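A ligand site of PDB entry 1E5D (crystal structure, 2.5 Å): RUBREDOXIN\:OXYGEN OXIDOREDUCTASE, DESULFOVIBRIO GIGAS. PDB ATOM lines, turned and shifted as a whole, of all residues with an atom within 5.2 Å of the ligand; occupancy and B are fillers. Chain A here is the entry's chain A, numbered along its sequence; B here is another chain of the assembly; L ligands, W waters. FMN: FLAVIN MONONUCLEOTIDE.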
ATOM      1  N   ASP A 260      26.038 -17.258 -19.053  1.00  0.00           N
ATOM      2  CA  ASP A 260      24.658 -16.798 -19.047  1.00  0.00           C
ATOM      3  C   ASP A 260      24.203 -16.802 -20.497  1.00  0.00           C
ATOM      4  O   ASP A 260      25.007 -16.956 -21.427  1.00  0.00           O
ATOM      5  CB  ASP A 260      24.505 -15.440 -18.394  1.00  0.00           C
ATOM      6  CG  ASP A 260      23.089 -15.186 -17.921  1.00  0.00           C
ATOM      7  OD1 ASP A 260      22.212 -16.049 -18.185  1.00  0.00           O
ATOM      8  OD2 ASP A 260      22.839 -14.129 -17.320  1.00  0.00           O
ATOM      9  N   SER A 261      22.904 -16.654 -20.715  1.00  0.00           N
ATOM     10  CA  SER A 261      22.369 -16.816 -22.069  1.00  0.00           C
ATOM     11  C   SER A 261      20.969 -16.235 -22.157  1.00  0.00           C
ATOM     12  O   SER A 261      20.254 -16.206 -21.148  1.00  0.00           O
ATOM     13  CB  SER A 261      22.376 -18.289 -22.428  1.00  0.00           C
ATOM     14  OG  SER A 261      21.870 -18.496 -23.737  1.00  0.00           O
ATOM     15  N   MET A 262      20.553 -15.773 -23.330  1.00  0.00           N
ATOM     16  CA  MET A 262      19.171 -15.298 -23.429  1.00  0.00           C
ATOM     17  C   MET A 262      18.316 -16.336 -24.158  1.00  0.00           C
ATOM     18  O   MET A 262      17.233 -16.649 -23.671  1.00  0.00           O
ATOM     19  CB  MET A 262      19.074 -13.934 -24.128  1.00  0.00           C
ATOM     20  CG  MET A 262      20.021 -12.913 -23.521  1.00  0.00           C
ATOM     21  SD  MET A 262      20.248 -11.445 -24.541  1.00  0.00           S
ATOM     22  CE  MET A 262      21.572 -11.990 -25.618  1.00  0.00           C
ATOM     23  N   TRP A 263      18.808 -16.838 -25.282  1.00  0.00           N
ATOM     24  CA  TRP A 263      18.034 -17.737 -26.133  1.00  0.00           C
ATOM     25  C   TRP A 263      18.643 -19.133 -26.205  1.00  0.00           C
ATOM     26  O   TRP A 263      18.378 -19.920 -27.116  1.00  0.00           O
ATOM     27  CB  TRP A 263      17.863 -17.119 -27.541  1.00  0.00           C
ATOM     28  CG  TRP A 263      16.886 -15.984 -27.449  1.00  0.00           C
ATOM     29  CD1 TRP A 263      17.147 -14.647 -27.475  1.00  0.00           C
ATOM     30  CD2 TRP A 263      15.458 -16.125 -27.305  1.00  0.00           C
ATOM     31  NE1 TRP A 263      15.964 -13.944 -27.360  1.00  0.00           N
ATOM     32  CE2 TRP A 263      14.920 -14.823 -27.254  1.00  0.00           C
ATOM     33  CE3 TRP A 263      14.597 -17.213 -27.214  1.00  0.00           C
ATOM     34  CZ2 TRP A 263      13.558 -14.578 -27.116  1.00  0.00           C
ATOM     35  CZ3 TRP A 263      13.251 -16.978 -27.088  1.00  0.00           C
ATOM     36  CH2 TRP A 263      12.733 -15.679 -27.039  1.00  0.00           C
ATOM     37  N   HIS A 264      19.460 -19.461 -25.223  1.00  0.00           N
ATOM     38  CA  HIS A 264      19.955 -20.810 -25.004  1.00  0.00           C
ATOM     39  C   HIS A 264      21.011 -21.291 -25.952  1.00  0.00           C
ATOM     40  O   HIS A 264      21.420 -22.450 -25.805  1.00  0.00           O
ATOM     41  CB  HIS A 264      18.763 -21.801 -25.055  1.00  0.00           C
ATOM     42  CG  HIS A 264      17.827 -21.392 -23.960  1.00  0.00           C
ATOM     43  ND1 HIS A 264      18.175 -21.530 -22.633  1.00  0.00           N
ATOM     44  CD2 HIS A 264      16.608 -20.819 -23.994  1.00  0.00           C
ATOM     45  CE1 HIS A 264      17.186 -21.081 -21.888  1.00  0.00           C
ATOM     46  NE2 HIS A 264      16.223 -20.639 -22.684  1.00  0.00           N
ATOM     47  N   SER A 265      21.483 -20.497 -26.918  1.00  0.00           N
ATOM     48  CA  SER A 265      22.518 -21.104 -27.769  1.00  0.00           C
ATOM     49  C   SER A 265      23.820 -21.178 -26.981  1.00  0.00           C
ATOM     50  O   SER A 265      24.563 -22.162 -27.045  1.00  0.00           O
ATOM     51  CB  SER A 265      22.708 -20.346 -29.072  1.00  0.00           C
ATOM     52  OG  SER A 265      21.550 -20.403 -29.890  1.00  0.00           O
ATOM     53  N   THR A 266      24.118 -20.125 -26.209  1.00  0.00           N
ATOM     54  CA  THR A 266      25.327 -20.220 -25.394  1.00  0.00           C
ATOM     55  C   THR A 266      25.167 -21.348 -24.375  1.00  0.00           C
ATOM     56  O   THR A 266      26.135 -21.977 -23.936  1.00  0.00           O
ATOM     57  CB  THR A 266      25.640 -18.890 -24.691  1.00  0.00           C
ATOM     58  OG1 THR A 266      25.790 -17.874 -25.698  1.00  0.00           O
ATOM     59  CG2 THR A 266      26.966 -18.969 -23.943  1.00  0.00           C
ATOM     60  N   GLU A 267      23.927 -21.646 -24.002  1.00  0.00           N
ATOM     61  CA  GLU A 267      23.737 -22.725 -23.042  1.00  0.00           C
ATOM     62  C   GLU A 267      24.073 -24.085 -23.633  1.00  0.00           C
ATOM     63  O   GLU A 267      24.761 -24.910 -23.007  1.00  0.00           O
ATOM     64  CB  GLU A 267      22.303 -22.728 -22.487  1.00  0.00           C
ATOM     65  CG  GLU A 267      22.170 -23.641 -21.284  1.00  0.00           C
ATOM     66  CD  GLU A 267      20.740 -24.087 -21.020  1.00  0.00           C
ATOM     67  OE1 GLU A 267      19.824 -23.300 -21.319  1.00  0.00           O
ATOM     68  OE2 GLU A 267      20.562 -25.204 -20.500  1.00  0.00           O
ATOM     69  N   PRO A 312      26.700 -14.783 -24.615  1.00  0.00           N
ATOM     70  CA  PRO A 312      26.330 -14.293 -25.939  1.00  0.00           C
ATOM     71  C   PRO A 312      26.727 -12.839 -26.039  1.00  0.00           C
ATOM     72  O   PRO A 312      27.009 -12.194 -25.031  1.00  0.00           O
ATOM     73  CB  PRO A 312      24.816 -14.451 -25.943  1.00  0.00           C
ATOM     74  CG  PRO A 312      24.427 -14.333 -24.509  1.00  0.00           C
ATOM     75  CD  PRO A 312      25.549 -14.990 -23.741  1.00  0.00           C
ATOM     76  N   THR A 313      26.756 -12.253 -27.227  1.00  0.00           N
ATOM     77  CA  THR A 313      27.027 -10.817 -27.246  1.00  0.00           C
ATOM     78  C   THR A 313      25.749 -10.036 -26.972  1.00  0.00           C
ATOM     79  O   THR A 313      24.736 -10.138 -27.654  1.00  0.00           O
ATOM     80  CB  THR A 313      27.613 -10.370 -28.593  1.00  0.00           C
ATOM     81  OG1 THR A 313      28.850 -11.067 -28.764  1.00  0.00           O
ATOM     82  CG2 THR A 313      27.924  -8.882 -28.546  1.00  0.00           C
ATOM     83  N   HIS A 314      25.795  -9.214 -25.915  1.00  0.00           N
ATOM     84  CA  HIS A 314      24.646  -8.390 -25.592  1.00  0.00           C
ATOM     85  C   HIS A 314      25.066  -6.929 -25.679  1.00  0.00           C
ATOM     86  O   HIS A 314      25.908  -6.530 -24.883  1.00  0.00           O
ATOM     87  CB  HIS A 314      24.095  -8.734 -24.211  1.00  0.00           C
ATOM     88  CG  HIS A 314      22.889  -7.945 -23.804  1.00  0.00           C
ATOM     89  ND1 HIS A 314      22.910  -6.990 -22.823  1.00  0.00           N
ATOM     90  CD2 HIS A 314      21.624  -7.967 -24.275  1.00  0.00           C
ATOM     91  CE1 HIS A 314      21.704  -6.460 -22.701  1.00  0.00           C
ATOM     92  NE2 HIS A 314      20.899  -7.036 -23.577  1.00  0.00           N
ATOM     93  N   ASN A 315      24.468  -6.209 -26.615  1.00  0.00           N
ATOM     94  CA  ASN A 315      24.813  -4.797 -26.807  1.00  0.00           C
ATOM     95  C   ASN A 315      26.313  -4.578 -26.838  1.00  0.00           C
ATOM     96  O   ASN A 315      26.873  -3.854 -26.013  1.00  0.00           O
ATOM     97  CB  ASN A 315      24.147  -3.953 -25.719  1.00  0.00           C
ATOM     98  CG  ASN A 315      22.640  -4.024 -25.792  1.00  0.00           C
ATOM     99  OD1 ASN A 315      22.025  -4.080 -26.852  1.00  0.00           O
ATOM    100  ND2 ASN A 315      22.019  -4.006 -24.619  1.00  0.00           N
ATOM    101  N   ASN A 316      26.975  -5.226 -27.794  1.00  0.00           N
ATOM    102  CA  ASN A 316      28.405  -4.998 -28.042  1.00  0.00           C
ATOM    103  C   ASN A 316      29.279  -5.429 -26.878  1.00  0.00           C
ATOM    104  O   ASN A 316      30.445  -5.041 -26.816  1.00  0.00           O
ATOM    105  CB  ASN A 316      28.633  -3.512 -28.359  1.00  0.00           C
ATOM    106  CG  ASN A 316      27.816  -3.160 -29.597  1.00  0.00           C
ATOM    107  OD1 ASN A 316      26.917  -2.320 -29.558  1.00  0.00           O
ATOM    108  ND2 ASN A 316      28.131  -3.842 -30.694  1.00  0.00           N
ATOM    109  N   GLY A 317      28.704  -6.222 -25.982  1.00  0.00           N
ATOM    110  CA  GLY A 317      29.439  -6.713 -24.840  1.00  0.00           C
ATOM    111  C   GLY A 317      28.868  -8.032 -24.343  1.00  0.00           C
ATOM    112  O   GLY A 317      28.198  -8.757 -25.076  1.00  0.00           O
ATOM    113  N   SER A 344      27.730 -17.103 -28.385  1.00  0.00           N
ATOM    114  CA  SER A 344      26.968 -16.901 -29.605  1.00  0.00           C
ATOM    115  C   SER A 344      26.795 -15.401 -29.800  1.00  0.00           C
ATOM    116  O   SER A 344      26.774 -14.650 -28.825  1.00  0.00           O
ATOM    117  CB  SER A 344      25.634 -17.623 -29.509  1.00  0.00           C
ATOM    118  OG  SER A 344      24.976 -17.661 -30.750  1.00  0.00           O
ATOM    119  N   PHE A 345      26.677 -14.950 -31.033  1.00  0.00           N
ATOM    120  CA  PHE A 345      26.590 -13.538 -31.365  1.00  0.00           C
ATOM    121  C   PHE A 345      25.710 -13.402 -32.596  1.00  0.00           C
ATOM    122  O   PHE A 345      25.485 -14.419 -33.265  1.00  0.00           O
ATOM    123  CB  PHE A 345      27.964 -12.910 -31.619  1.00  0.00           C
ATOM    124  CG  PHE A 345      28.574 -13.418 -32.916  1.00  0.00           C
ATOM    125  CD1 PHE A 345      29.131 -14.682 -32.960  1.00  0.00           C
ATOM    126  CD2 PHE A 345      28.556 -12.631 -34.061  1.00  0.00           C
ATOM    127  CE1 PHE A 345      29.657 -15.162 -34.156  1.00  0.00           C
ATOM    128  CE2 PHE A 345      29.073 -13.109 -35.255  1.00  0.00           C
ATOM    129  CZ  PHE A 345      29.619 -14.379 -35.292  1.00  0.00           C
ATOM    130  N   GLY A 346      25.229 -12.200 -32.872  1.00  0.00           N
ATOM    131  CA  GLY A 346      24.327 -11.993 -33.997  1.00  0.00           C
ATOM    132  C   GLY A 346      24.947 -11.171 -35.116  1.00  0.00           C
ATOM    133  O   GLY A 346      24.590 -11.300 -36.284  1.00  0.00           O
ATOM    134  N   TRP A 347      25.891 -10.296 -34.768  1.00  0.00           N
ATOM    135  CA  TRP A 347      26.534  -9.476 -35.795  1.00  0.00           C
ATOM    136  C   TRP A 347      27.888  -8.957 -35.321  1.00  0.00           C
ATOM    137  O   TRP A 347      28.913  -9.264 -35.935  1.00  0.00           O
ATOM    138  CB  TRP A 347      25.645  -8.318 -36.202  1.00  0.00           C
ATOM    139  CG  TRP A 347      25.087  -7.444 -35.124  1.00  0.00           C
ATOM    140  CD1 TRP A 347      25.623  -6.282 -34.642  1.00  0.00           C
ATOM    141  CD2 TRP A 347      23.873  -7.660 -34.385  1.00  0.00           C
ATOM    142  NE1 TRP A 347      24.828  -5.756 -33.657  1.00  0.00           N
ATOM    143  CE2 TRP A 347      23.752  -6.593 -33.474  1.00  0.00           C
ATOM    144  CE3 TRP A 347      22.901  -8.655 -34.408  1.00  0.00           C
ATOM    145  CZ2 TRP A 347      22.675  -6.486 -32.586  1.00  0.00           C
ATOM    146  CZ3 TRP A 347      21.831  -8.556 -33.530  1.00  0.00           C
ATOM    147  CH2 TRP A 347      21.741  -7.477 -32.634  1.00  0.00           C
ATOM    148  N   SER A 348      27.908  -8.167 -34.261  1.00  0.00           N
ATOM    149  CA  SER A 348      29.162  -7.560 -33.815  1.00  0.00           C
ATOM    150  C   SER A 348      30.098  -8.610 -33.235  1.00  0.00           C
ATOM    151  O   SER A 348      31.286  -8.613 -33.563  1.00  0.00           O
ATOM    152  CB  SER A 348      28.901  -6.425 -32.824  1.00  0.00           C
ATOM    153  OG  SER A 348      27.949  -6.746 -31.835  1.00  0.00           O
ATOM    154  N   GLY A 349      29.597  -9.514 -32.387  1.00  0.00           N
ATOM    155  CA  GLY A 349      30.388 -10.631 -31.933  1.00  0.00           C
ATOM    156  C   GLY A 349      31.493 -10.338 -30.947  1.00  0.00           C
ATOM    157  O   GLY A 349      32.465 -11.091 -30.878  1.00  0.00           O
ATOM    158  N   GLU A 350      31.408  -9.263 -30.147  1.00  0.00           N
ATOM    159  CA  GLU A 350      32.479  -8.944 -29.217  1.00  0.00           C
ATOM    160  C   GLU A 350      32.636  -9.889 -28.034  1.00  0.00           C
ATOM    161  O   GLU A 350      33.708  -9.860 -27.418  1.00  0.00           O
ATOM    162  CB  GLU A 350      32.248  -7.537 -28.611  1.00  0.00           C
ATOM    163  CG  GLU A 350      32.454  -6.404 -29.596  1.00  0.00           C
ATOM    164  CD  GLU A 350      31.150  -5.912 -30.187  1.00  0.00           C
ATOM    165  OE1 GLU A 350      30.246  -6.744 -30.391  1.00  0.00           O
ATOM    166  OE2 GLU A 350      31.066  -4.693 -30.447  1.00  0.00           O
ATOM    167  N   ASN A 375      24.575 -17.055 -33.895  1.00  0.00           N
ATOM    168  CA  ASN A 375      23.283 -17.617 -33.511  1.00  0.00           C
ATOM    169  C   ASN A 375      23.346 -19.087 -33.124  1.00  0.00           C
ATOM    170  O   ASN A 375      24.138 -19.453 -32.257  1.00  0.00           O
ATOM    171  CB  ASN A 375      22.286 -17.405 -34.662  1.00  0.00           C
ATOM    172  CG  ASN A 375      22.172 -15.911 -34.929  1.00  0.00           C
ATOM    173  OD1 ASN A 375      22.255 -15.452 -36.064  1.00  0.00           O
ATOM    174  ND2 ASN A 375      21.958 -15.176 -33.844  1.00  0.00           N
ATOM    175  N   VAL A 376      22.508 -19.897 -33.759  1.00  0.00           N
ATOM    176  CA  VAL A 376      22.279 -21.267 -33.320  1.00  0.00           C
ATOM    177  C   VAL A 376      23.303 -22.224 -33.901  1.00  0.00           C
ATOM    178  O   VAL A 376      23.438 -22.391 -35.104  1.00  0.00           O
ATOM    179  CB  VAL A 376      20.858 -21.745 -33.669  1.00  0.00           C
ATOM    180  CG1 VAL A 376      20.663 -23.195 -33.238  1.00  0.00           C
ATOM    181  CG2 VAL A 376      19.848 -20.834 -32.991  1.00  0.00           C
ATOM    182  N   TYR B  26      17.464 -10.811 -20.416  1.00  0.00           N
ATOM    183  CA  TYR B  26      18.228  -9.561 -20.256  1.00  0.00           C
ATOM    184  C   TYR B  26      17.502  -8.566 -19.368  1.00  0.00           C
ATOM    185  O   TYR B  26      18.130  -7.793 -18.641  1.00  0.00           O
ATOM    186  CB  TYR B  26      18.546  -8.944 -21.626  1.00  0.00           C
ATOM    187  CG  TYR B  26      17.390  -8.396 -22.400  1.00  0.00           C
ATOM    188  CD1 TYR B  26      16.618  -9.213 -23.218  1.00  0.00           C
ATOM    189  CD2 TYR B  26      17.047  -7.050 -22.344  1.00  0.00           C
ATOM    190  CE1 TYR B  26      15.554  -8.712 -23.940  1.00  0.00           C
ATOM    191  CE2 TYR B  26      15.989  -6.530 -23.054  1.00  0.00           C
ATOM    192  CZ  TYR B  26      15.242  -7.378 -23.860  1.00  0.00           C
ATOM    193  OH  TYR B  26      14.178  -6.876 -24.581  1.00  0.00           O
ATOM    194  N   GLU B  81      14.352 -13.163 -34.179  1.00  0.00           N
ATOM    195  CA  GLU B  81      14.468 -13.538 -32.775  1.00  0.00           C
ATOM    196  C   GLU B  81      13.471 -14.662 -32.504  1.00  0.00           C
ATOM    197  O   GLU B  81      12.347 -14.652 -33.033  1.00  0.00           O
ATOM    198  CB  GLU B  81      14.217 -12.334 -31.878  1.00  0.00           C
ATOM    199  CG  GLU B  81      14.761 -12.525 -30.474  1.00  0.00           C
ATOM    200  CD  GLU B  81      14.851 -11.197 -29.735  1.00  0.00           C
ATOM    201  OE1 GLU B  81      14.931 -10.142 -30.420  1.00  0.00           O
ATOM    202  OE2 GLU B  81      14.818 -11.214 -28.504  1.00  0.00           O
ATOM    203  N   HIS B 113      19.787 -19.250 -37.702  1.00  0.00           N
ATOM    204  CA  HIS B 113      18.958 -19.751 -36.620  1.00  0.00           C
ATOM    205  C   HIS B 113      18.383 -21.123 -36.936  1.00  0.00           C
ATOM    206  O   HIS B 113      18.294 -21.990 -36.076  1.00  0.00           O
ATOM    207  CB  HIS B 113      17.811 -18.789 -36.325  1.00  0.00           C
ATOM    208  CG  HIS B 113      18.153 -17.643 -35.441  1.00  0.00           C
ATOM    209  ND1 HIS B 113      18.688 -16.467 -35.925  1.00  0.00           N
ATOM    210  CD2 HIS B 113      18.048 -17.482 -34.097  1.00  0.00           C
ATOM    211  CE1 HIS B 113      18.892 -15.640 -34.925  1.00  0.00           C
ATOM    212  NE2 HIS B 113      18.514 -16.229 -33.799  1.00  0.00           N
ATOM    213  N   HIS B 146      15.027  -3.943 -33.364  1.00  0.00           N
ATOM    214  CA  HIS B 146      16.286  -3.759 -32.666  1.00  0.00           C
ATOM    215  C   HIS B 146      17.324  -4.747 -33.182  1.00  0.00           C
ATOM    216  O   HIS B 146      18.399  -4.883 -32.597  1.00  0.00           O
ATOM    217  CB  HIS B 146      16.103  -3.957 -31.148  1.00  0.00           C
ATOM    218  CG  HIS B 146      15.655  -5.376 -30.875  1.00  0.00           C
ATOM    219  ND1 HIS B 146      16.515  -6.384 -30.519  1.00  0.00           N
ATOM    220  CD2 HIS B 146      14.432  -5.941 -30.942  1.00  0.00           C
ATOM    221  CE1 HIS B 146      15.833  -7.505 -30.358  1.00  0.00           C
ATOM    222  NE2 HIS B 146      14.559  -7.260 -30.607  1.00  0.00           N
ATOM    223  N   TRP B 147      16.990  -5.438 -34.269  1.00  0.00           N
ATOM    224  CA  TRP B 147      17.971  -6.324 -34.895  1.00  0.00           C
ATOM    225  C   TRP B 147      18.184  -5.918 -36.345  1.00  0.00           C
ATOM    226  O   TRP B 147      17.349  -5.205 -36.910  1.00  0.00           O
ATOM    227  CB  TRP B 147      17.537  -7.785 -34.829  1.00  0.00           C
ATOM    228  CG  TRP B 147      17.937  -8.490 -33.571  1.00  0.00           C
ATOM    229  CD1 TRP B 147      18.359  -7.932 -32.400  1.00  0.00           C
ATOM    230  CD2 TRP B 147      17.954  -9.913 -33.359  1.00  0.00           C
ATOM    231  NE1 TRP B 147      18.636  -8.917 -31.479  1.00  0.00           N
ATOM    232  CE2 TRP B 147      18.394 -10.143 -32.048  1.00  0.00           C
ATOM    233  CE3 TRP B 147      17.632 -11.003 -34.174  1.00  0.00           C
ATOM    234  CZ2 TRP B 147      18.521 -11.430 -31.538  1.00  0.00           C
ATOM    235  CZ3 TRP B 147      17.761 -12.277 -33.661  1.00  0.00           C
ATOM    236  CH2 TRP B 147      18.208 -12.480 -32.345  1.00  0.00           C
ATOM    237  N   ILE B 197      15.862  -2.079 -24.488  1.00  0.00           N
ATOM    238  CA  ILE B 197      16.273  -2.838 -25.671  1.00  0.00           C
ATOM    239  C   ILE B 197      16.498  -1.932 -26.870  1.00  0.00           C
ATOM    240  O   ILE B 197      17.446  -2.163 -27.621  1.00  0.00           O
ATOM    241  CB  ILE B 197      15.260  -3.934 -26.055  1.00  0.00           C
ATOM    242  CG1 ILE B 197      15.478  -4.542 -27.439  1.00  0.00           C
ATOM    243  CG2 ILE B 197      13.839  -3.398 -25.940  1.00  0.00           C
ATOM    244  CD1 ILE B 197      15.628  -6.039 -27.410  1.00  0.00           C
ATOM    245  N   TYR B 201      19.896   2.188 -30.189  1.00  0.00           N
ATOM    246  CA  TYR B 201      19.575   2.544 -31.563  1.00  0.00           C
ATOM    247  C   TYR B 201      18.560   3.684 -31.597  1.00  0.00           C
ATOM    248  O   TYR B 201      17.650   3.734 -32.415  1.00  0.00           O
ATOM    249  CB  TYR B 201      19.038   1.312 -32.316  1.00  0.00           C
ATOM    250  CG  TYR B 201      19.895   0.103 -31.991  1.00  0.00           C
ATOM    251  CD1 TYR B 201      21.179  -0.008 -32.506  1.00  0.00           C
ATOM    252  CD2 TYR B 201      19.404  -0.896 -31.158  1.00  0.00           C
ATOM    253  CE1 TYR B 201      21.959  -1.111 -32.215  1.00  0.00           C
ATOM    254  CE2 TYR B 201      20.185  -1.999 -30.867  1.00  0.00           C
ATOM    255  CZ  TYR B 201      21.461  -2.092 -31.392  1.00  0.00           C
ATOM    256  OH  TYR B 201      22.233  -3.196 -31.085  1.00  0.00           O
HETATM  257  N1  FMN L   1      24.533  -9.808 -31.187  1.00  0.00           N
HETATM  258  C2  FMN L   1      25.559  -9.063 -31.591  1.00  0.00           C
HETATM  259  O2  FMN L   1      26.300  -9.411 -32.479  1.00  0.00           O
HETATM  260  N3  FMN L   1      25.862  -7.813 -30.993  1.00  0.00           N
HETATM  261  C4  FMN L   1      24.905  -7.150 -30.246  1.00  0.00           C
HETATM  262  O4  FMN L   1      25.218  -6.100 -29.730  1.00  0.00           O
HETATM  263  C4A FMN L   1      23.747  -7.939 -29.839  1.00  0.00           C
HETATM  264  N5  FMN L   1      22.956  -7.517 -28.827  1.00  0.00           N
HETATM  265  C5A FMN L   1      21.738  -8.135 -28.718  1.00  0.00           C
HETATM  266  C6  FMN L   1      20.823  -7.631 -27.749  1.00  0.00           C
HETATM  267  C7  FMN L   1      19.695  -8.336 -27.391  1.00  0.00           C
HETATM  268  C7M FMN L   1      18.922  -7.923 -26.172  1.00  0.00           C
HETATM  269  C8  FMN L   1      19.445  -9.636 -27.984  1.00  0.00           C
HETATM  270  C8M FMN L   1      18.105 -10.313 -27.782  1.00  0.00           C
HETATM  271  C9  FMN L   1      20.228 -10.040 -29.078  1.00  0.00           C
HETATM  272  C9A FMN L   1      21.455  -9.409 -29.295  1.00  0.00           C
HETATM  273  N10 FMN L   1      22.494  -9.975 -30.101  1.00  0.00           N
HETATM  274  C10 FMN L   1      23.567  -9.256 -30.428  1.00  0.00           C
HETATM  275  C1' FMN L   1      22.206 -11.270 -30.747  1.00  0.00           C
HETATM  276  C2' FMN L   1      22.510 -12.453 -29.794  1.00  0.00           C
HETATM  277  O2' FMN L   1      23.892 -12.442 -29.431  1.00  0.00           O
HETATM  278  C3' FMN L   1      22.179 -13.708 -30.587  1.00  0.00           C
HETATM  279  O3' FMN L   1      20.761 -13.832 -30.542  1.00  0.00           O
HETATM  280  C4' FMN L   1      22.809 -14.946 -29.940  1.00  0.00           C
HETATM  281  O4' FMN L   1      22.449 -16.114 -30.696  1.00  0.00           O
HETATM  282  C5' FMN L   1      22.294 -15.032 -28.525  1.00  0.00           C
HETATM  283  O5' FMN L   1      22.901 -16.311 -27.835  1.00  0.00           O
HETATM  284  P   FMN L   1      22.166 -17.000 -26.696  1.00  0.00           P
HETATM  285  O1P FMN L   1      23.234 -17.810 -25.951  1.00  0.00           O
HETATM  286  O2P FMN L   1      21.436 -16.108 -25.911  1.00  0.00           O
HETATM  287  O3P FMN L   1      21.193 -17.930 -27.243  1.00  0.00           O
HETATM  288  O   HOH W   1      18.950  -5.845 -29.934  1.00  0.00           O
HETATM  289  O   HOH W   2      19.671 -15.946 -31.355  1.00  0.00           O
HETATM  290  O   HOH W   3      21.168 -12.345 -33.791  1.00  0.00           O
HETATM  291  O   HOH W   4      20.473 -17.989 -29.897  1.00  0.00           O
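N of Trp 347 is in hydrogen-bond range of O2 of the ligand, at 2.5 Å.
The backbone NH (N) of Ser 348 sits at hydrogen-bond distance from an oxygen (O2) of the ligand (2.7 Å).
The side-chain hydroxyl of Ser 348 sits at hydrogen-bond distance from a nitrogen (N3) of the ligand, 2.5 Å away.
O1P of the ligand sits at hydrogen-bond distance from N of Thr 266 (2.5 Å).
An oxygen (O1P) of the ligand is in hydrogen-bond range of the side-chain hydroxyl (OG1) of Thr 266 (2.6 Å).
The backbone NH (N) of Ser 265 lies within hydrogen-bond range of an oxygen (O3P) of the ligand, 2.6 Å away.
O1P of the ligand lies within hydrogen-bond range of OG of Ser 261, 2.7 Å away.
The backbone NH of Met 262 lies within hydrogen-bond range of an oxygen (O2P) of the ligand, at 2.7 Å.
N of Asn 316 sits at hydrogen-bond distance from O4 of the ligand (2.8 Å).
O2P of the ligand lies within hydrogen-bond range of N of Trp 263 (2.8 Å).
OG of Ser 344 lies within hydrogen-bond range of O4' of the ligand (3.0 Å).
The backbone NH of Asn 315 sits at hydrogen-bond distance from a nitrogen (N5) of the ligand (3.0 Å).
N of Gly 346 sits at hydrogen-bond distance from N1 of the ligand (3.0 Å).
O2' of the ligand lies within hydrogen-bond range of O of Thr 313.
An oxygen (O3P) of the ligand sits at hydrogen-bond distance from the backbone NH of His 264, 3.1 Å away.
ND2 of Asn 375 lies close to O4' of the ligand, at 3.3 Å.
N of Gly 349 lies within hydrogen-bond range of O2 of the ligand, at 3.3 Å.
ND2 of Asn 316 is in hydrogen-bond range of OG of Ser 348 (3.1 Å).
The indole nitrogen (NE1) of Trp 263 lies within hydrogen-bond range of the side-chain carboxylate (OE2) of Glu 81 of chain B (3.2 Å).
The backbone carbonyl oxygen (O) of Ser 344 sits at hydrogen-bond distance from the backbone NH (N) of Thr 313 (2.9 Å).
The backbone carbonyl oxygen of Asn 375 sits at hydrogen-bond distance from the side-chain hydroxyl of Ser 344 (2.5 Å).
ND2 of Asn 315 lies close to NE2 of His 314 (3.4 Å).
A ring nitrogen (ND1) of His 264 sits at hydrogen-bond distance from the side-chain carboxylate (OE1) of Glu 267, at 2.8 Å.
The indole nitrogen (NE1) of Trp 147 of chain B sits close to a ring nitrogen (ND1) of His 146 of chain B.
The backbone NH (N) of Asn 375 sits at hydrogen-bond distance from the backbone carbonyl oxygen (O) of Phe 345 (2.9 Å).
Pro 312 touches the ligand (CB to O5', 3.3 Å).
CD2 of His 314 touches C7M of the ligand (3.3 Å).
CA of Phe 345 touches O2' of the ligand, at 3.5 Å.
CD1 of Tyr 26 of chain B touches C7M of the ligand, at 3.96 Å.
OE2 of Glu 81 of chain B touches C8M of the ligand (3.5 Å).
Trp 147 of chain B touches the ligand (NE1 to C9, 3.1 Å).
Ile 197 of chain B touches the ligand.
Hydrophobic or aromatic side chains within 4 Å of the ligand: Met 262, Trp 263, Pro 312, His 314, Phe 345, Trp 347, Tyr 26 of chain B, Trp 147 of chain B and Ile 197 of chain B.
Within 4 Å of the ligand: Ser 261, Met 262, Trp 263, His 264, Ser 265, Thr 266, Pro 312, Thr 313, His 314, Asn 315, Asn 316, Ser 344, Phe 345, Gly 346, Trp 347, Ser 348, Gly 349, Asn 375, Tyr 26 of chain B, Glu 81 of chain B, Trp 147 of chain B and Ile 197 of chain B.
Along chain A the residues within 4 Å of the ligand span positions 261 to 375.
Water W2 lies within hydrogen-bond range of O3' of the ligand, NE2 of His 113 of chain B and ND2 of Asn 375.
Water W4 lies within hydrogen-bond range of OG of Ser 265 and O3P of the ligand.
Water W1 lies within hydrogen-bond range of a ring nitrogen (ND1) of His 146 of chain B (2.6 Å) and the indole nitrogen of Trp 147 of chain B (3.5 Å).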
